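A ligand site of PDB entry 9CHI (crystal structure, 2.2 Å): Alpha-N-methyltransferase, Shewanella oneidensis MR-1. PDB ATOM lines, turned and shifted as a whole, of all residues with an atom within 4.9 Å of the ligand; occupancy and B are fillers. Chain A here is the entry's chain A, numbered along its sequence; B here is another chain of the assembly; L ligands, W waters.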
ATOM      1  N   LEU A  10      -4.909  33.467  12.561  1.00  0.00           N
ATOM      2  CA  LEU A  10      -4.410  33.173  11.242  1.00  0.00           C
ATOM      3  C   LEU A  10      -3.250  34.113  10.896  1.00  0.00           C
ATOM      4  O   LEU A  10      -2.318  33.727  10.209  1.00  0.00           O
ATOM      5  CB  LEU A  10      -5.537  33.273  10.213  1.00  0.00           C
ATOM      6  CG  LEU A  10      -6.474  32.064  10.152  1.00  0.00           C
ATOM      7  CD1 LEU A  10      -7.630  32.320   9.191  1.00  0.00           C
ATOM      8  CD2 LEU A  10      -5.715  30.808   9.758  1.00  0.00           C
ATOM      9  N   TYR A  92      -3.177  27.059  15.345  1.00  0.00           N
ATOM     10  CA  TYR A  92      -3.512  28.236  14.575  1.00  0.00           C
ATOM     11  C   TYR A  92      -5.020  28.440  14.607  1.00  0.00           C
ATOM     12  O   TYR A  92      -5.770  27.484  14.770  1.00  0.00           O
ATOM     13  CB  TYR A  92      -2.972  28.102  13.146  1.00  0.00           C
ATOM     14  CG  TYR A  92      -3.713  27.097  12.272  1.00  0.00           C
ATOM     15  CD1 TYR A  92      -3.411  25.744  12.317  1.00  0.00           C
ATOM     16  CD2 TYR A  92      -4.706  27.500  11.392  1.00  0.00           C
ATOM     17  CE1 TYR A  92      -4.077  24.823  11.521  1.00  0.00           C
ATOM     18  CE2 TYR A  92      -5.378  26.598  10.588  1.00  0.00           C
ATOM     19  CZ  TYR A  92      -5.060  25.251  10.665  1.00  0.00           C
ATOM     20  OH  TYR A  92      -5.731  24.351   9.877  1.00  0.00           O
ATOM     21  N   GLY A  93      -5.447  29.697  14.475  1.00  0.00           N
ATOM     22  CA  GLY A  93      -6.850  30.055  14.568  1.00  0.00           C
ATOM     23  C   GLY A  93      -7.419  29.696  15.940  1.00  0.00           C
ATOM     24  O   GLY A  93      -6.754  29.888  16.963  1.00  0.00           O
ATOM     25  N   HIS A  94      -8.638  29.161  15.944  1.00  0.00           N
ATOM     26  CA  HIS A  94      -9.306  28.754  17.175  1.00  0.00           C
ATOM     27  C   HIS A  94      -8.978  27.284  17.440  1.00  0.00           C
ATOM     28  O   HIS A  94      -9.142  26.436  16.571  1.00  0.00           O
ATOM     29  CB  HIS A  94     -10.816  29.033  17.057  1.00  0.00           C
ATOM     30  CG  HIS A  94     -11.589  28.781  18.305  1.00  0.00           C
ATOM     31  ND1 HIS A  94     -11.346  27.730  19.171  1.00  0.00           N
ATOM     32  CD2 HIS A  94     -12.651  29.429  18.819  1.00  0.00           C
ATOM     33  CE1 HIS A  94     -12.212  27.773  20.165  1.00  0.00           C
ATOM     34  NE2 HIS A  94     -13.017  28.793  19.971  1.00  0.00           N
ATOM     35  N   VAL A  97     -11.999  24.764  16.831  1.00  0.00           N
ATOM     36  CA  VAL A  97     -12.820  24.883  15.629  1.00  0.00           C
ATOM     37  C   VAL A  97     -12.230  23.961  14.562  1.00  0.00           C
ATOM     38  O   VAL A  97     -11.101  24.158  14.112  1.00  0.00           O
ATOM     39  CB  VAL A  97     -12.906  26.338  15.132  1.00  0.00           C
ATOM     40  CG1 VAL A  97     -13.579  26.425  13.768  1.00  0.00           C
ATOM     41  CG2 VAL A  97     -13.616  27.235  16.138  1.00  0.00           C
ATOM     42  N   PHE A  98     -13.016  22.957  14.165  1.00  0.00           N
ATOM     43  CA  PHE A  98     -12.569  21.949  13.216  1.00  0.00           C
ATOM     44  C   PHE A  98     -11.186  21.450  13.640  1.00  0.00           C
ATOM     45  O   PHE A  98     -10.315  21.230  12.810  1.00  0.00           O
ATOM     46  CB  PHE A  98     -12.590  22.526  11.799  1.00  0.00           C
ATOM     47  CG  PHE A  98     -13.991  22.660  11.203  1.00  0.00           C
ATOM     48  CD1 PHE A  98     -14.827  23.709  11.566  1.00  0.00           C
ATOM     49  CD2 PHE A  98     -14.463  21.735  10.271  1.00  0.00           C
ATOM     50  CE1 PHE A  98     -16.095  23.825  11.032  1.00  0.00           C
ATOM     51  CE2 PHE A  98     -15.732  21.858   9.730  1.00  0.00           C
ATOM     52  CZ  PHE A  98     -16.545  22.897  10.111  1.00  0.00           C
ATOM     53  N   ALA A  99     -11.010  21.299  14.962  1.00  0.00           N
ATOM     54  CA  ALA A  99      -9.772  20.789  15.521  1.00  0.00           C
ATOM     55  C   ALA A  99     -10.100  19.871  16.705  1.00  0.00           C
ATOM     56  O   ALA A  99     -10.558  20.334  17.740  1.00  0.00           O
ATOM     57  CB  ALA A  99      -8.891  21.946  15.951  1.00  0.00           C
ATOM     58  N   ILE A 122      -9.229  33.392  17.300  1.00  0.00           N
ATOM     59  CA  ILE A 122      -9.841  33.881  16.084  1.00  0.00           C
ATOM     60  C   ILE A 122      -9.679  32.830  14.993  1.00  0.00           C
ATOM     61  O   ILE A 122      -8.563  32.525  14.586  1.00  0.00           O
ATOM     62  CB  ILE A 122      -9.220  35.236  15.687  1.00  0.00           C
ATOM     63  CG1 ILE A 122      -9.360  36.270  16.803  1.00  0.00           C
ATOM     64  CG2 ILE A 122      -9.812  35.745  14.366  1.00  0.00           C
ATOM     65  CD1 ILE A 122      -8.579  37.549  16.576  1.00  0.00           C
ATOM     66  N   SER A 123     -10.810  32.278  14.531  1.00  0.00           N
ATOM     67  CA  SER A 123     -10.810  31.210  13.541  1.00  0.00           C
ATOM     68  C   SER A 123     -10.823  31.809  12.131  1.00  0.00           C
ATOM     69  O   SER A 123     -10.934  33.021  11.971  1.00  0.00           O
ATOM     70  CB  SER A 123     -11.981  30.285  13.749  1.00  0.00           C
ATOM     71  OG  SER A 123     -13.210  30.935  13.464  1.00  0.00           O
ATOM     72  N   ALA A 124     -10.729  30.929  11.138  1.00  0.00           N
ATOM     73  CA  ALA A 124     -10.757  31.334   9.736  1.00  0.00           C
ATOM     74  C   ALA A 124     -12.131  31.890   9.394  1.00  0.00           C
ATOM     75  O   ALA A 124     -12.262  32.703   8.474  1.00  0.00           O
ATOM     76  CB  ALA A 124     -10.399  30.159   8.851  1.00  0.00           C
ATOM     77  N   GLU A 125     -13.139  31.452  10.150  1.00  0.00           N
ATOM     78  CA  GLU A 125     -14.503  31.930   9.969  1.00  0.00           C
ATOM     79  C   GLU A 125     -14.574  33.384  10.403  1.00  0.00           C
ATOM     80  O   GLU A 125     -15.134  34.222   9.689  1.00  0.00           O
ATOM     81  CB  GLU A 125     -15.456  31.053  10.785  1.00  0.00           C
ATOM     82  CG  GLU A 125     -16.907  31.482  10.699  1.00  0.00           C
ATOM     83  CD  GLU A 125     -17.818  30.753  11.671  1.00  0.00           C
ATOM     84  OE1 GLU A 125     -17.860  29.511  11.627  1.00  0.00           O
ATOM     85  OE2 GLU A 125     -18.484  31.438  12.483  1.00  0.00           O
ATOM     86  N   LEU A 164     -18.299  25.394   3.590  1.00  0.00           N
ATOM     87  CA  LEU A 164     -17.804  24.038   3.499  1.00  0.00           C
ATOM     88  C   LEU A 164     -16.297  24.043   3.752  1.00  0.00           C
ATOM     89  O   LEU A 164     -15.524  24.479   2.906  1.00  0.00           O
ATOM     90  CB  LEU A 164     -18.133  23.420   2.136  1.00  0.00           C
ATOM     91  CG  LEU A 164     -19.617  23.310   1.794  1.00  0.00           C
ATOM     92  CD1 LEU A 164     -19.813  22.495   0.527  1.00  0.00           C
ATOM     93  CD2 LEU A 164     -20.408  22.705   2.951  1.00  0.00           C
ATOM     94  N   TRP A 165     -15.900  23.571   4.937  1.00  0.00           N
ATOM     95  CA  TRP A 165     -14.495  23.573   5.330  1.00  0.00           C
ATOM     96  C   TRP A 165     -13.775  22.384   4.696  1.00  0.00           C
ATOM     97  O   TRP A 165     -14.414  21.434   4.234  1.00  0.00           O
ATOM     98  CB  TRP A 165     -14.360  23.541   6.851  1.00  0.00           C
ATOM     99  CG  TRP A 165     -15.041  24.687   7.554  1.00  0.00           C
ATOM    100  CD1 TRP A 165     -16.328  25.112   7.388  1.00  0.00           C
ATOM    101  CD2 TRP A 165     -14.454  25.562   8.543  1.00  0.00           C
ATOM    102  NE1 TRP A 165     -16.584  26.180   8.207  1.00  0.00           N
ATOM    103  CE2 TRP A 165     -15.457  26.483   8.929  1.00  0.00           C
ATOM    104  CE3 TRP A 165     -13.191  25.660   9.132  1.00  0.00           C
ATOM    105  CZ2 TRP A 165     -15.230  27.480   9.870  1.00  0.00           C
ATOM    106  CZ3 TRP A 165     -12.966  26.647  10.063  1.00  0.00           C
ATOM    107  CH2 TRP A 165     -13.971  27.548  10.430  1.00  0.00           C
ATOM    108  N   GLN A 166     -12.436  22.457   4.687  1.00  0.00           N
ATOM    109  CA  GLN A 166     -11.604  21.410   4.116  1.00  0.00           C
ATOM    110  C   GLN A 166     -12.186  20.968   2.779  1.00  0.00           C
ATOM    111  O   GLN A 166     -12.405  19.775   2.553  1.00  0.00           O
ATOM    112  CB  GLN A 166     -11.499  20.244   5.100  1.00  0.00           C
ATOM    113  CG  GLN A 166     -10.809  20.595   6.415  1.00  0.00           C
ATOM    114  CD  GLN A 166     -10.618  19.410   7.335  1.00  0.00           C
ATOM    115  OE1 GLN A 166     -11.072  18.293   7.052  1.00  0.00           O
ATOM    116  NE2 GLN A 166      -9.951  19.640   8.450  1.00  0.00           N
ATOM    117  N   ILE A 167     -12.415  21.934   1.886  1.00  0.00           N
ATOM    118  CA  ILE A 167     -12.966  21.657   0.568  1.00  0.00           C
ATOM    119  C   ILE A 167     -11.905  20.978  -0.282  1.00  0.00           C
ATOM    120  O   ILE A 167     -12.220  20.360  -1.298  1.00  0.00           O
ATOM    121  CB  ILE A 167     -13.484  22.962  -0.084  1.00  0.00           C
ATOM    122  CG1 ILE A 167     -14.185  22.684  -1.412  1.00  0.00           C
ATOM    123  CG2 ILE A 167     -12.349  23.971  -0.252  1.00  0.00           C
ATOM    124  CD1 ILE A 167     -15.457  21.864  -1.279  1.00  0.00           C
ATOM    125  N   TYR A 205     -12.274  31.245  -0.307  1.00  0.00           N
ATOM    126  CA  TYR A 205     -11.654  32.182   0.602  1.00  0.00           C
ATOM    127  C   TYR A 205     -10.396  31.569   1.214  1.00  0.00           C
ATOM    128  O   TYR A 205     -10.363  30.382   1.512  1.00  0.00           O
ATOM    129  CB  TYR A 205     -12.657  32.618   1.688  1.00  0.00           C
ATOM    130  CG  TYR A 205     -12.032  33.448   2.800  1.00  0.00           C
ATOM    131  CD1 TYR A 205     -11.693  34.785   2.604  1.00  0.00           C
ATOM    132  CD2 TYR A 205     -11.810  32.901   4.057  1.00  0.00           C
ATOM    133  CE1 TYR A 205     -11.131  35.535   3.613  1.00  0.00           C
ATOM    134  CE2 TYR A 205     -11.246  33.654   5.083  1.00  0.00           C
ATOM    135  CZ  TYR A 205     -10.904  34.972   4.855  1.00  0.00           C
ATOM    136  OH  TYR A 205     -10.350  35.717   5.860  1.00  0.00           O
ATOM    137  N   GLU A 206      -9.374  32.411   1.389  1.00  0.00           N
ATOM    138  CA  GLU A 206      -8.161  32.021   2.093  1.00  0.00           C
ATOM    139  C   GLU A 206      -7.646  33.216   2.881  1.00  0.00           C
ATOM    140  O   GLU A 206      -7.102  34.158   2.309  1.00  0.00           O
ATOM    141  CB  GLU A 206      -7.087  31.534   1.122  1.00  0.00           C
ATOM    142  CG  GLU A 206      -7.468  30.254   0.373  1.00  0.00           C
ATOM    143  CD  GLU A 206      -6.386  29.758  -0.578  1.00  0.00           C
ATOM    144  OE1 GLU A 206      -5.331  30.420  -0.661  1.00  0.00           O
ATOM    145  OE2 GLU A 206      -6.605  28.717  -1.228  1.00  0.00           O
ATOM    146  N   ALA A 207      -7.814  33.156   4.206  1.00  0.00           N
ATOM    147  CA  ALA A 207      -7.333  34.217   5.087  1.00  0.00           C
ATOM    148  C   ALA A 207      -5.818  34.319   4.961  1.00  0.00           C
ATOM    149  O   ALA A 207      -5.127  33.318   4.802  1.00  0.00           O
ATOM    150  CB  ALA A 207      -7.752  33.929   6.509  1.00  0.00           C
ATOM    151  N   ASN A 209      -2.002  34.795   6.124  1.00  0.00           N
ATOM    152  CA  ASN A 209      -1.216  34.366   7.264  1.00  0.00           C
ATOM    153  C   ASN A 209      -0.132  35.388   7.571  1.00  0.00           C
ATOM    154  O   ASN A 209       0.476  35.361   8.634  1.00  0.00           O
ATOM    155  CB  ASN A 209      -0.599  32.983   7.031  1.00  0.00           C
ATOM    156  CG  ASN A 209      -1.648  31.900   6.916  1.00  0.00           C
ATOM    157  OD1 ASN A 209      -2.374  31.635   7.884  1.00  0.00           O
ATOM    158  ND2 ASN A 209      -1.742  31.268   5.752  1.00  0.00           N
ATOM    159  N   PRO A 232      -5.115  23.285   1.075  1.00  0.00           N
ATOM    160  CA  PRO A 232      -5.633  22.803   2.354  1.00  0.00           C
ATOM    161  C   PRO A 232      -6.374  23.874   3.153  1.00  0.00           C
ATOM    162  O   PRO A 232      -7.345  23.577   3.849  1.00  0.00           O
ATOM    163  CB  PRO A 232      -4.366  22.317   3.088  1.00  0.00           C
ATOM    164  CG  PRO A 232      -3.421  21.926   1.964  1.00  0.00           C
ATOM    165  CD  PRO A 232      -3.701  22.933   0.862  1.00  0.00           C
ATOM    166  N   ILE A 233      -5.911  25.127   3.038  1.00  0.00           N
ATOM    167  CA  ILE A 233      -6.423  26.218   3.848  1.00  0.00           C
ATOM    168  C   ILE A 233      -7.595  26.887   3.135  1.00  0.00           C
ATOM    169  O   ILE A 233      -8.029  27.961   3.521  1.00  0.00           O
ATOM    170  CB  ILE A 233      -5.310  27.225   4.166  1.00  0.00           C
ATOM    171  CG1 ILE A 233      -4.801  27.922   2.901  1.00  0.00           C
ATOM    172  CG2 ILE A 233      -4.167  26.565   4.945  1.00  0.00           C
ATOM    173  CD1 ILE A 233      -3.755  28.990   3.155  1.00  0.00           C
ATOM    174  N   SER A 234      -8.099  26.235   2.078  1.00  0.00           N
ATOM    175  CA  SER A 234      -9.184  26.787   1.291  1.00  0.00           C
ATOM    176  C   SER A 234     -10.526  26.505   1.960  1.00  0.00           C
ATOM    177  O   SER A 234     -10.811  25.370   2.349  1.00  0.00           O
ATOM    178  CB  SER A 234      -9.165  26.262  -0.122  1.00  0.00           C
ATOM    179  OG  SER A 234      -7.995  26.691  -0.809  1.00  0.00           O
ATOM    180  N   THR A 235     -11.346  27.554   2.086  1.00  0.00           N
ATOM    181  CA  THR A 235     -12.718  27.424   2.570  1.00  0.00           C
ATOM    182  C   THR A 235     -13.665  27.853   1.462  1.00  0.00           C
ATOM    183  O   THR A 235     -13.425  28.852   0.791  1.00  0.00           O
ATOM    184  CB  THR A 235     -12.897  28.263   3.832  1.00  0.00           C
ATOM    185  OG1 THR A 235     -11.897  27.820   4.743  1.00  0.00           O
ATOM    186  CG2 THR A 235     -14.275  28.084   4.450  1.00  0.00           C
ATOM    187  N   LEU B  61      -2.065  21.308   7.589  1.00  0.00           N
ATOM    188  CA  LEU B  61      -2.858  22.139   8.492  1.00  0.00           C
ATOM    189  C   LEU B  61      -4.231  21.513   8.733  1.00  0.00           C
ATOM    190  O   LEU B  61      -5.112  22.161   9.295  1.00  0.00           O
ATOM    191  CB  LEU B  61      -2.980  23.548   7.924  1.00  0.00           C
ATOM    192  CG  LEU B  61      -2.151  24.632   8.621  1.00  0.00           C
ATOM    193  CD1 LEU B  61      -0.660  24.398   8.490  1.00  0.00           C
ATOM    194  CD2 LEU B  61      -2.535  26.004   8.096  1.00  0.00           C
ATOM    195  N   IML B  63      -6.634  19.433  10.821  1.00  0.00           N
ATOM    196  CA  IML B  63      -6.681  18.876  12.176  1.00  0.00           C
ATOM    197  C   IML B  63      -8.056  18.265  12.474  1.00  0.00           C
ATOM    198  O   IML B  63      -8.526  18.323  13.605  1.00  0.00           O
ATOM    199  CB  IML B  63      -6.299  19.953  13.217  1.00  0.00           C
ATOM    200  CN  IML B  63      -7.611  20.474  10.516  1.00  0.00           C
ATOM    201  CG2 IML B  63      -5.945  19.327  14.559  1.00  0.00           C
ATOM    202  CG1 IML B  63      -5.183  20.863  12.704  1.00  0.00           C
ATOM    203  CD1 IML B  63      -4.968  22.106  13.535  1.00  0.00           C
ATOM    204  N   SER B  64      -8.662  17.660  11.453  1.00  0.00           N
ATOM    205  CA  SER B  64      -9.994  17.080  11.570  1.00  0.00           C
ATOM    206  C   SER B  64     -10.337  16.263  10.335  1.00  0.00           C
ATOM    207  O   SER B  64      -9.624  16.306   9.333  1.00  0.00           O
ATOM    208  CB  SER B  64     -11.022  18.156  11.829  1.00  0.00           C
ATOM    209  OG  SER B  64     -11.029  19.116  10.781  1.00  0.00           O
HETATM  210  N1  LIG L   1      -8.707  25.803  13.759  1.00  0.00           N
HETATM  211  C1  LIG L   1      -8.724  26.467  12.425  1.00  0.00           C
HETATM  212  C2  LIG L   1      -9.293  25.527  11.358  1.00  0.00           C
HETATM  213  C3  LIG L   1      -8.725  24.116  11.406  1.00  0.00           C
HETATM  214  S1  LIG L   1      -9.511  22.996  10.229  1.00  0.00           S
HETATM  215  C4  LIG L   1      -9.589  27.726  12.492  1.00  0.00           C
HETATM  216  O1  LIG L   1      -9.869  28.162  13.634  1.00  0.00           O
HETATM  217  O2  LIG L   1      -9.955  28.220  11.412  1.00  0.00           O
HETATM  218  C5  LIG L   1      -8.753  23.495   8.665  1.00  0.00           C
HETATM  219  C6  LIG L   1      -9.713  24.131   7.702  1.00  0.00           C
HETATM  220  O3  LIG L   1      -9.975  25.495   8.112  1.00  0.00           O
HETATM  221  C7  LIG L   1      -9.218  24.246   6.265  1.00  0.00           C
HETATM  222  O4  LIG L   1      -9.465  23.042   5.542  1.00  0.00           O
HETATM  223  C8  LIG L   1     -10.044  25.421   5.748  1.00  0.00           C
HETATM  224  O5  LIG L   1     -11.364  25.034   5.397  1.00  0.00           O
HETATM  225  C9  LIG L   1     -10.038  26.330   6.974  1.00  0.00           C
HETATM  226  N2  LIG L   1      -8.911  27.257   7.006  1.00  0.00           N
HETATM  227  C10 LIG L   1      -7.733  27.072   7.686  1.00  0.00           C
HETATM  228  N3  LIG L   1      -6.889  28.062   7.526  1.00  0.00           N
HETATM  229  C11 LIG L   1      -7.542  28.946   6.694  1.00  0.00           C
HETATM  230  C12 LIG L   1      -7.173  30.193   6.146  1.00  0.00           C
HETATM  231  N4  LIG L   1      -6.003  30.783   6.379  1.00  0.00           N
HETATM  232  N5  LIG L   1      -8.070  30.823   5.356  1.00  0.00           N
HETATM  233  C13 LIG L   1      -9.248  30.228   5.119  1.00  0.00           C
HETATM  234  N6  LIG L   1      -9.700  29.060   5.565  1.00  0.00           N
HETATM  235  C14 LIG L   1      -8.795  28.459   6.355  1.00  0.00           C
HETATM  236  O   HOH W   1      -6.502  24.801  14.361  1.00  0.00           O
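N of Ala 207 lies within hydrogen-bond range of N5 of the ligand (2.6 Å). The backbone carbonyl oxygen (O) of Ala 207 lies within hydrogen-bond range of a nitrogen (N4) of the ligand (3.1 Å). N6 of the ligand sits at hydrogen-bond distance from OG1 of Thr 235 (2.7 Å). An oxygen (O4) of the ligand is in hydrogen-bond range of the backbone carbonyl oxygen (O) of Pro 232 (2.8 Å). An oxygen (O1) of the ligand is in hydrogen-bond range of the backbone NH of His 94. The backbone carbonyl oxygen of His 94 sits at hydrogen-bond distance from a nitrogen (N1) of the ligand, at 2.9 Å. O2 of the ligand lies within hydrogen-bond range of N of Ala 124, at 2.8 Å. O5 of the ligand lies within hydrogen-bond range of N of Gln 166 (2.9 Å). A nitrogen (N1) of the ligand sits at hydrogen-bond distance from the backbone carbonyl oxygen of Val 97. The backbone carbonyl oxygen of Ser 234 sits at hydrogen-bond distance from an oxygen (O5) of the ligand, 3.1 Å away.
N of Tyr 205 lies within hydrogen-bond range of O of Thr 235, at 2.9 Å. The side-chain amide nitrogen of Gln 166 is in hydrogen-bond range of the side-chain hydroxyl of Ser 64 of chain B (2.6 Å). The side-chain hydroxyl (OG) of Ser 123 lies close to the backbone NH (N) of Glu 125, 3.4 Å away. OE2 of Glu 206 is in hydrogen-bond range of OG of Ser 234 (2.5 Å). The side-chain hydroxyl (OG) of Ser 64 of chain B is in hydrogen-bond range of the backbone carbonyl oxygen (O) of Phe 98, at 3.0 Å. O of Leu 10 sits close to OD1 of Asn 209.
The backbone carbonyl oxygen (O) of Phe 98 lies close to a sulfur (S1) of the ligand (3.2 Å). O of Ile 233 sits close to N6 of the ligand (2.9 Å). Residues that only touch the ligand: Ser 123, IML 63 of chain B, Tyr 92, Trp 165, Leu 10, Glu 206, Gly 93, Tyr 205 and Leu 61 of chain B. Hydrophobic or aromatic side chains within 4 Å of the ligand: Leu 10, Tyr 92, His 94, Val 97, Phe 98, Ala 124, Trp 165, Tyr 205, Ala 207 and Ile 233.
Water W1 lies within hydrogen-bond range of a nitrogen (N1) of the ligand (2.5 Å) and the backbone carbonyl oxygen (O) of Tyr 92 (2.8 Å).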
